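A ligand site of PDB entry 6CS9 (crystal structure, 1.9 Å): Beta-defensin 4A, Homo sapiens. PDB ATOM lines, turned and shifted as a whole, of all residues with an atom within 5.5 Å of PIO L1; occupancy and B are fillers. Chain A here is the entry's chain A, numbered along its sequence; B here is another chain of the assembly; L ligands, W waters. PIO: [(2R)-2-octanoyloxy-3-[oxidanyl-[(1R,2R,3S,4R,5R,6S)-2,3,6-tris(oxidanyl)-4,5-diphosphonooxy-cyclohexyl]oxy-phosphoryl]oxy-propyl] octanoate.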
ATOM      1  N   PRO A   5      17.362  21.488  29.600  1.00  0.00           N
ATOM      2  CA  PRO A   5      16.890  20.200  29.059  1.00  0.00           C
ATOM      3  C   PRO A   5      16.080  20.345  27.784  1.00  0.00           C
ATOM      4  O   PRO A   5      16.137  19.455  26.928  1.00  0.00           O
ATOM      5  CB  PRO A   5      16.050  19.618  30.207  1.00  0.00           C
ATOM      6  CG  PRO A   5      15.556  20.811  30.939  1.00  0.00           C
ATOM      7  CD  PRO A   5      16.605  21.880  30.813  1.00  0.00           C
ATOM      8  N   VAL A   6      15.328  21.434  27.614  1.00  0.00           N
ATOM      9  CA  VAL A   6      14.549  21.621  26.391  1.00  0.00           C
ATOM     10  C   VAL A   6      15.483  21.708  25.192  1.00  0.00           C
ATOM     11  O   VAL A   6      15.314  20.983  24.202  1.00  0.00           O
ATOM     12  CB  VAL A   6      13.655  22.868  26.501  1.00  0.00           C
ATOM     13  CG1 VAL A   6      12.997  23.163  25.161  1.00  0.00           C
ATOM     14  CG2 VAL A   6      12.607  22.674  27.587  1.00  0.00           C
ATOM     15  N   CYS A   8      18.531  20.750  24.931  1.00  0.00           N
ATOM     16  CA  CYS A   8      19.262  19.492  24.759  1.00  0.00           C
ATOM     17  C   CYS A   8      18.460  18.504  23.925  1.00  0.00           C
ATOM     18  O   CYS A   8      18.938  17.986  22.912  1.00  0.00           O
ATOM     19  CB  CYS A   8      19.595  18.905  26.123  1.00  0.00           C
ATOM     20  SG  CYS A   8      20.515  17.371  26.028  1.00  0.00           S
ATOM     21  N   LEU A   9      17.222  18.237  24.342  1.00  0.00           N
ATOM     22  CA  LEU A   9      16.406  17.259  23.632  1.00  0.00           C
ATOM     23  C   LEU A   9      15.957  17.755  22.265  1.00  0.00           C
ATOM     24  O   LEU A   9      15.654  16.925  21.396  1.00  0.00           O
ATOM     25  CB  LEU A   9      15.189  16.893  24.487  1.00  0.00           C
ATOM     26  CG  LEU A   9      15.503  16.094  25.742  1.00  0.00           C
ATOM     27  CD1 LEU A   9      14.290  16.040  26.639  1.00  0.00           C
ATOM     28  CD2 LEU A   9      15.957  14.694  25.360  1.00  0.00           C
ATOM     29  N   LYS A  10      15.916  19.068  22.049  1.00  0.00           N
ATOM     30  CA  LYS A  10      15.589  19.606  20.737  1.00  0.00           C
ATOM     31  C   LYS A  10      16.799  19.656  19.811  1.00  0.00           C
ATOM     32  O   LYS A  10      16.653  20.071  18.654  1.00  0.00           O
ATOM     33  CB  LYS A  10      14.975  20.999  20.865  1.00  0.00           C
ATOM     34  CG  LYS A  10      13.640  21.020  21.606  1.00  0.00           C
ATOM     35  CD  LYS A  10      12.530  20.342  20.827  1.00  0.00           C
ATOM     36  CE  LYS A  10      12.139  21.135  19.588  1.00  0.00           C
ATOM     37  NZ  LYS A  10      11.017  20.498  18.867  1.00  0.00           N
ATOM     38  N   SER A  11      17.984  19.254  20.290  1.00  0.00           N
ATOM     39  CA  SER A  11      19.198  19.244  19.488  1.00  0.00           C
ATOM     40  C   SER A  11      19.653  17.832  19.142  1.00  0.00           C
ATOM     41  O   SER A  11      20.832  17.608  18.887  1.00  0.00           O
ATOM     42  CB  SER A  11      20.313  19.990  20.219  1.00  0.00           C
ATOM     43  OG  SER A  11      19.899  21.280  20.630  1.00  0.00           O
ATOM     44  N   GLY A  12      18.725  16.874  19.127  1.00  0.00           N
ATOM     45  CA  GLY A  12      19.066  15.501  18.827  1.00  0.00           C
ATOM     46  C   GLY A  12      19.890  14.807  19.893  1.00  0.00           C
ATOM     47  O   GLY A  12      20.660  13.896  19.580  1.00  0.00           O
ATOM     48  N   ALA A  13      19.750  15.223  21.147  1.00  0.00           N
ATOM     49  CA  ALA A  13      20.556  14.708  22.241  1.00  0.00           C
ATOM     50  C   ALA A  13      19.661  14.221  23.371  1.00  0.00           C
ATOM     51  O   ALA A  13      18.432  14.375  23.326  1.00  0.00           O
ATOM     52  CB  ALA A  13      21.552  15.764  22.749  1.00  0.00           C
ATOM     53  N   CYS A  15      19.455  13.757  27.881  1.00  0.00           N
ATOM     54  CA  CYS A  15      19.937  14.096  29.209  1.00  0.00           C
ATOM     55  C   CYS A  15      20.259  12.820  29.964  1.00  0.00           C
ATOM     56  O   CYS A  15      19.450  11.896  30.000  1.00  0.00           O
ATOM     57  CB  CYS A  15      18.889  14.909  29.981  1.00  0.00           C
ATOM     58  SG  CYS A  15      18.488  16.469  29.208  1.00  0.00           S
ATOM     59  N   LEU A  32      20.039  20.226  35.159  1.00  0.00           N
ATOM     60  CA  LEU A  32      19.689  19.507  36.377  1.00  0.00           C
ATOM     61  C   LEU A  32      20.949  18.994  37.054  1.00  0.00           C
ATOM     62  O   LEU A  32      21.988  18.808  36.408  1.00  0.00           O
ATOM     63  CB  LEU A  32      18.770  18.343  36.042  1.00  0.00           C
ATOM     64  CG  LEU A  32      17.455  18.699  35.329  1.00  0.00           C
ATOM     65  CD1 LEU A  32      16.694  17.439  34.933  1.00  0.00           C
ATOM     66  CD2 LEU A  32      16.598  19.585  36.220  1.00  0.00           C
ATOM     67  N   LYS A  39      25.156  13.348  23.038  1.00  0.00           N
ATOM     68  CA  LYS A  39      24.778  13.150  21.646  1.00  0.00           C
ATOM     69  C   LYS A  39      25.757  12.211  20.970  1.00  0.00           C
ATOM     70  O   LYS A  39      26.970  12.338  21.134  1.00  0.00           O
ATOM     71  CB  LYS A  39      24.751  14.494  20.902  1.00  0.00           C
ATOM     72  CG  LYS A  39      24.222  14.414  19.479  1.00  0.00           C
ATOM     73  CD  LYS A  39      24.065  15.816  18.895  1.00  0.00           C
ATOM     74  CE  LYS A  39      23.307  15.796  17.571  1.00  0.00           C
ATOM     75  NZ  LYS A  39      22.965  17.185  17.131  1.00  0.00           N
ATOM     76  N   HIS B  16      17.104   7.622  31.601  1.00  0.00           N
ATOM     77  CA  HIS B  16      16.730   8.998  31.237  1.00  0.00           C
ATOM     78  C   HIS B  16      15.734   9.576  32.234  1.00  0.00           C
ATOM     79  O   HIS B  16      14.799   8.885  32.655  1.00  0.00           O
ATOM     80  CB  HIS B  16      16.123   9.040  29.827  1.00  0.00           C
ATOM     81  CG  HIS B  16      16.179  10.398  29.204  1.00  0.00           C
ATOM     82  ND1 HIS B  16      15.142  11.305  29.301  1.00  0.00           N
ATOM     83  CD2 HIS B  16      17.159  11.005  28.485  1.00  0.00           C
ATOM     84  CE1 HIS B  16      15.478  12.421  28.668  1.00  0.00           C
ATOM     85  NE2 HIS B  16      16.700  12.257  28.167  1.00  0.00           N
ATOM     86  N   PRO B  17      15.902  10.836  32.654  1.00  0.00           N
ATOM     87  CA  PRO B  17      14.962  11.399  33.623  1.00  0.00           C
ATOM     88  C   PRO B  17      13.582  11.630  33.022  1.00  0.00           C
ATOM     89  O   PRO B  17      13.450  12.021  31.854  1.00  0.00           O
ATOM     90  CB  PRO B  17      15.612  12.734  34.028  1.00  0.00           C
ATOM     91  CG  PRO B  17      17.055  12.592  33.650  1.00  0.00           C
ATOM     92  CD  PRO B  17      17.066  11.708  32.435  1.00  0.00           C
ATOM     93  N   VAL B  18      12.559  11.373  33.828  1.00  0.00           N
ATOM     94  CA  VAL B  18      11.171  11.722  33.527  1.00  0.00           C
ATOM     95  C   VAL B  18      10.530  10.790  32.496  1.00  0.00           C
ATOM     96  O   VAL B  18       9.514  10.155  32.785  1.00  0.00           O
ATOM     97  CB  VAL B  18      11.061  13.192  33.058  1.00  0.00           C
ATOM     98  CG1 VAL B  18       9.615  13.585  32.913  1.00  0.00           C
ATOM     99  CG2 VAL B  18      11.756  14.118  34.049  1.00  0.00           C
ATOM    100  N   PHE B  19      11.104  10.709  31.302  1.00  0.00           N
ATOM    101  CA  PHE B  19      10.517   9.920  30.235  1.00  0.00           C
ATOM    102  C   PHE B  19      11.615   9.445  29.288  1.00  0.00           C
ATOM    103  O   PHE B  19      12.744   9.936  29.317  1.00  0.00           O
ATOM    104  CB  PHE B  19       9.462  10.725  29.456  1.00  0.00           C
ATOM    105  CG  PHE B  19      10.024  11.932  28.765  1.00  0.00           C
ATOM    106  CD1 PHE B  19      10.050  13.162  29.406  1.00  0.00           C
ATOM    107  CD2 PHE B  19      10.541  11.842  27.486  1.00  0.00           C
ATOM    108  CE1 PHE B  19      10.572  14.273  28.767  1.00  0.00           C
ATOM    109  CE2 PHE B  19      11.070  12.948  26.850  1.00  0.00           C
ATOM    110  CZ  PHE B  19      11.084  14.160  27.488  1.00  0.00           C
ATOM    111  N   ARG B  22      12.501  10.420  22.357  1.00  0.00           N
ATOM    112  CA  ARG B  22      11.959   9.933  21.097  1.00  0.00           C
ATOM    113  C   ARG B  22      12.818   8.812  20.536  1.00  0.00           C
ATOM    114  O   ARG B  22      14.044   8.906  20.515  1.00  0.00           O
ATOM    115  CB  ARG B  22      11.887  11.082  20.103  1.00  0.00           C
ATOM    116  CG  ARG B  22      13.227  11.773  19.883  1.00  0.00           C
ATOM    117  CD  ARG B  22      13.076  12.989  18.986  1.00  0.00           C
ATOM    118  NE  ARG B  22      12.105  12.738  17.923  1.00  0.00           N
ATOM    119  CZ  ARG B  22      12.410  12.172  16.761  1.00  0.00           C
ATOM    120  NH1 ARG B  22      13.654  11.807  16.490  1.00  0.00           N
ATOM    121  NH2 ARG B  22      11.454  11.981  15.864  1.00  0.00           N
HETATM  122  C1  PIO L   1      13.593  16.778  17.941  1.00  0.00           C
HETATM  123  O1  PIO L   1      13.200  17.132  19.244  1.00  0.00           O
HETATM  124  P1  PIO L   1      11.749  16.588  19.802  1.00  0.00           P
HETATM  125  C2  PIO L   1      14.887  15.951  18.029  1.00  0.00           C
HETATM  126  O2  PIO L   1      15.832  16.674  18.780  1.00  0.00           O
HETATM  127  C3  PIO L   1      15.450  15.658  16.630  1.00  0.00           C
HETATM  128  O3  PIO L   1      16.662  14.963  16.757  1.00  0.00           O
HETATM  129  C4  PIO L   1      15.685  16.954  15.844  1.00  0.00           C
HETATM  130  O4  PIO L   1      16.146  16.629  14.552  1.00  0.00           O
HETATM  131  P4  PIO L   1      17.702  17.002  14.152  1.00  0.00           P
HETATM  132  C5  PIO L   1      14.387  17.761  15.732  1.00  0.00           C
HETATM  133  O5  PIO L   1      14.670  18.973  15.082  1.00  0.00           O
HETATM  134  P5  PIO L   1      13.553  19.587  14.039  1.00  0.00           P
HETATM  135  C6  PIO L   1      13.799  18.061  17.116  1.00  0.00           C
HETATM  136  O6  PIO L   1      12.557  18.704  16.971  1.00  0.00           O
HETATM  137  O11 PIO L   1      11.320  15.384  18.997  1.00  0.00           O
HETATM  138  O12 PIO L   1      10.710  17.675  19.650  1.00  0.00           O
HETATM  139  O13 PIO L   1      11.896  16.144  21.380  1.00  0.00           O
HETATM  140  C1A PIO L   1      11.548  18.445  25.074  1.00  0.00           C
HETATM  141  O1A PIO L   1      11.705  19.221  24.203  1.00  0.00           O
HETATM  142  C1B PIO L   1       8.679  14.671  24.402  1.00  0.00           C
HETATM  143  O1B PIO L   1       8.048  13.671  24.504  1.00  0.00           O
HETATM  144  C1C PIO L   1      11.938  17.100  22.400  1.00  0.00           C
HETATM  145  C2A PIO L   1      11.298  18.968  26.495  1.00  0.00           C
HETATM  146  C2B PIO L   1       8.643  15.735  25.496  1.00  0.00           C
HETATM  147  C2C PIO L   1      11.021  16.694  23.557  1.00  0.00           C
HETATM  148  O2C PIO L   1      11.581  17.078  24.792  1.00  0.00           O
HETATM  149  C3A PIO L   1      11.276  17.836  27.517  1.00  0.00           C
HETATM  150  C3B PIO L   1       7.596  15.415  26.561  1.00  0.00           C
HETATM  151  C3C PIO L   1      10.804  15.174  23.591  1.00  0.00           C
HETATM  152  O3C PIO L   1       9.472  14.889  23.278  1.00  0.00           O
HETATM  153  O41 PIO L   1      18.641  16.105  14.927  1.00  0.00           O
HETATM  154  O42 PIO L   1      17.979  18.452  14.489  1.00  0.00           O
HETATM  155  O43 PIO L   1      17.888  16.779  12.678  1.00  0.00           O
HETATM  156  C4A PIO L   1      11.455  18.431  28.922  1.00  0.00           C
HETATM  157  C4B PIO L   1       6.720  16.643  26.822  1.00  0.00           C
HETATM  158  O51 PIO L   1      14.017  20.933  13.537  1.00  0.00           O
HETATM  159  O52 PIO L   1      12.218  19.735  14.724  1.00  0.00           O
HETATM  160  O53 PIO L   1      13.390  18.647  12.856  1.00  0.00           O
HETATM  161  C5A PIO L   1      12.732  17.901  29.595  1.00  0.00           C
HETATM  162  C5B PIO L   1       6.737  17.008  28.306  1.00  0.00           C
HETATM  163  C6A PIO L   1      12.386  16.858  30.653  1.00  0.00           C
HETATM  164  C6B PIO L   1       6.248  18.450  28.495  1.00  0.00           C
HETATM  165  C7A PIO L   1      13.424  15.734  30.672  1.00  0.00           C
HETATM  166  C7B PIO L   1       4.786  18.609  28.067  1.00  0.00           C
HETATM  167  C8A PIO L   1      14.606  16.132  31.543  1.00  0.00           C
HETATM  168  C8B PIO L   1       4.540  20.001  27.492  1.00  0.00           C
HETATM  169  C1  PIO L   2       5.605   6.611  38.166  1.00  0.00           C
HETATM  170  O1  PIO L   2       6.716   6.897  37.359  1.00  0.00           O
HETATM  171  P1  PIO L   2       7.750   8.083  37.841  1.00  0.00           P
HETATM  172  C2  PIO L   2       5.919   5.385  39.039  1.00  0.00           C
HETATM  173  O2  PIO L   2       6.290   4.314  38.195  1.00  0.00           O
HETATM  174  C3  PIO L   2       4.703   4.948  39.867  1.00  0.00           C
HETATM  175  O3  PIO L   2       5.017   3.744  40.500  1.00  0.00           O
HETATM  176  C4  PIO L   2       3.450   4.741  39.014  1.00  0.00           C
HETATM  177  O4  PIO L   2       2.361   4.560  39.877  1.00  0.00           O
HETATM  178  P4  PIO L   2       1.906   3.014  40.258  1.00  0.00           P
HETATM  179  C5  PIO L   2       3.160   5.928  38.092  1.00  0.00           C
HETATM  180  O5  PIO L   2       2.145   5.544  37.195  1.00  0.00           O
HETATM  181  P5  PIO L   2       1.059   6.662  36.667  1.00  0.00           P
HETATM  182  C6  PIO L   2       4.384   6.352  37.279  1.00  0.00           C
HETATM  183  O6  PIO L   2       4.096   7.536  36.566  1.00  0.00           O
HETATM  184  O11 PIO L   2       9.060   7.892  37.122  1.00  0.00           O
HETATM  185  O12 PIO L   2       7.981   7.978  39.336  1.00  0.00           O
HETATM  186  O13 PIO L   2       7.113   9.569  37.503  1.00  0.00           O
HETATM  187  C1A PIO L   2       6.088  12.648  36.467  1.00  0.00           C
HETATM  188  O1A PIO L   2       5.361  11.920  37.030  1.00  0.00           O
HETATM  189  C1B PIO L   2      11.044  13.420  38.521  1.00  0.00           C
HETATM  190  O1B PIO L   2      11.052  13.495  39.706  1.00  0.00           O
HETATM  191  C1C PIO L   2       7.847  10.463  36.707  1.00  0.00           C
HETATM  192  C2A PIO L   2       5.641  13.359  35.194  1.00  0.00           C
HETATM  193  C2B PIO L   2      12.345  13.311  37.721  1.00  0.00           C
HETATM  194  C2C PIO L   2       8.067  11.774  37.473  1.00  0.00           C
HETATM  195  O2C PIO L   2       7.378  12.867  36.960  1.00  0.00           O
HETATM  196  C3A PIO L   2       6.579  14.502  34.777  1.00  0.00           C
HETATM  197  C3B PIO L   2      13.557  13.535  38.628  1.00  0.00           C
HETATM  198  C3C PIO L   2       9.554  12.118  37.363  1.00  0.00           C
HETATM  199  O3C PIO L   2       9.813  13.401  37.847  1.00  0.00           O
HETATM  200  O41 PIO L   2       1.332   2.355  39.027  1.00  0.00           O
HETATM  201  O42 PIO L   2       0.866   3.055  41.347  1.00  0.00           O
HETATM  202  O43 PIO L   2       3.109   2.222  40.723  1.00  0.00           O
HETATM  203  C4A PIO L   2       7.082  15.330  35.966  1.00  0.00           C
HETATM  204  C4B PIO L   2      14.507  14.562  38.018  1.00  0.00           C
HETATM  205  O51 PIO L   2      -0.203   5.947  36.257  1.00  0.00           O
HETATM  206  O52 PIO L   2       1.633   7.412  35.499  1.00  0.00           O
HETATM  207  O53 PIO L   2       0.734   7.641  37.772  1.00  0.00           O
HETATM  208  C5A PIO L   2       7.034  16.819  35.642  1.00  0.00           C
HETATM  209  C5B PIO L   2      15.912  13.968  37.977  1.00  0.00           C
HETATM  210  C6A PIO L   2       8.125  17.199  34.632  1.00  0.00           C
HETATM  211  C6B PIO L   2      16.903  15.037  37.506  1.00  0.00           C
HETATM  212  C7A PIO L   2       7.507  17.876  33.415  1.00  0.00           C
HETATM  213  C7B PIO L   2      18.251  14.832  38.184  1.00  0.00           C
HETATM  214  C8A PIO L   2       8.566  18.692  32.677  1.00  0.00           C
HETATM  215  C8B PIO L   2      19.044  13.746  37.456  1.00  0.00           C
HETATM  216  O   HOH W   1      16.549  20.543  13.651  1.00  0.00           O
HETATM  217  O   HOH W   2      16.851  21.108  16.068  1.00  0.00           O
HETATM  218  O   HOH W   3      19.892  18.922  12.434  1.00  0.00           O
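The backbone carbonyl oxygen of Leu 9 is in hydrogen-bond range of an oxygen (O2) of PIO L1 (2.6 Å).
O2 of PIO L1 lies within hydrogen-bond range of N of Gly 12 (2.9 Å).
An oxygen (O2) of PIO L1 lies close to the backbone carbonyl oxygen (O) of Lys 10 (3.5 Å).
The side-chain amino group of Lys 10 is in salt-bridge range of an oxygen (O12) of PIO L1, at 2.9 Å.
The guanidinium group (NE) of Arg 22 of chain B is in salt-bridge range of an oxygen (O11) of PIO L1 (3.0 Å).
A ring nitrogen (ND1) of His 16 of chain B lies within hydrogen-bond range of the backbone carbonyl oxygen (O) of Phe 19 of chain B (2.8 Å).
The side-chain amino group (NZ) of Lys 39 lies within hydrogen-bond range of the backbone carbonyl oxygen (O) of Ser 11, at 2.8 Å.
Merely in contact with PIO L1: Phe 19 of chain B, Ser 11, Pro 5 and Pro 17 of chain B.
Hydrophobic or aromatic side chains within 4 Å of PIO L1: Pro 5, Leu 9 and Phe 19 of chain B.
Eight residues have an atom within 4 Å of PIO L1: Pro 5, Leu 9, Lys 10, Ser 11, Gly 12, Pro 17 of chain B, Phe 19 of chain B and Arg 22 of chain B.
Water W2 bridges O of Lys 10 (2.8 Å) and O5 of PIO L1 (3.2 Å).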
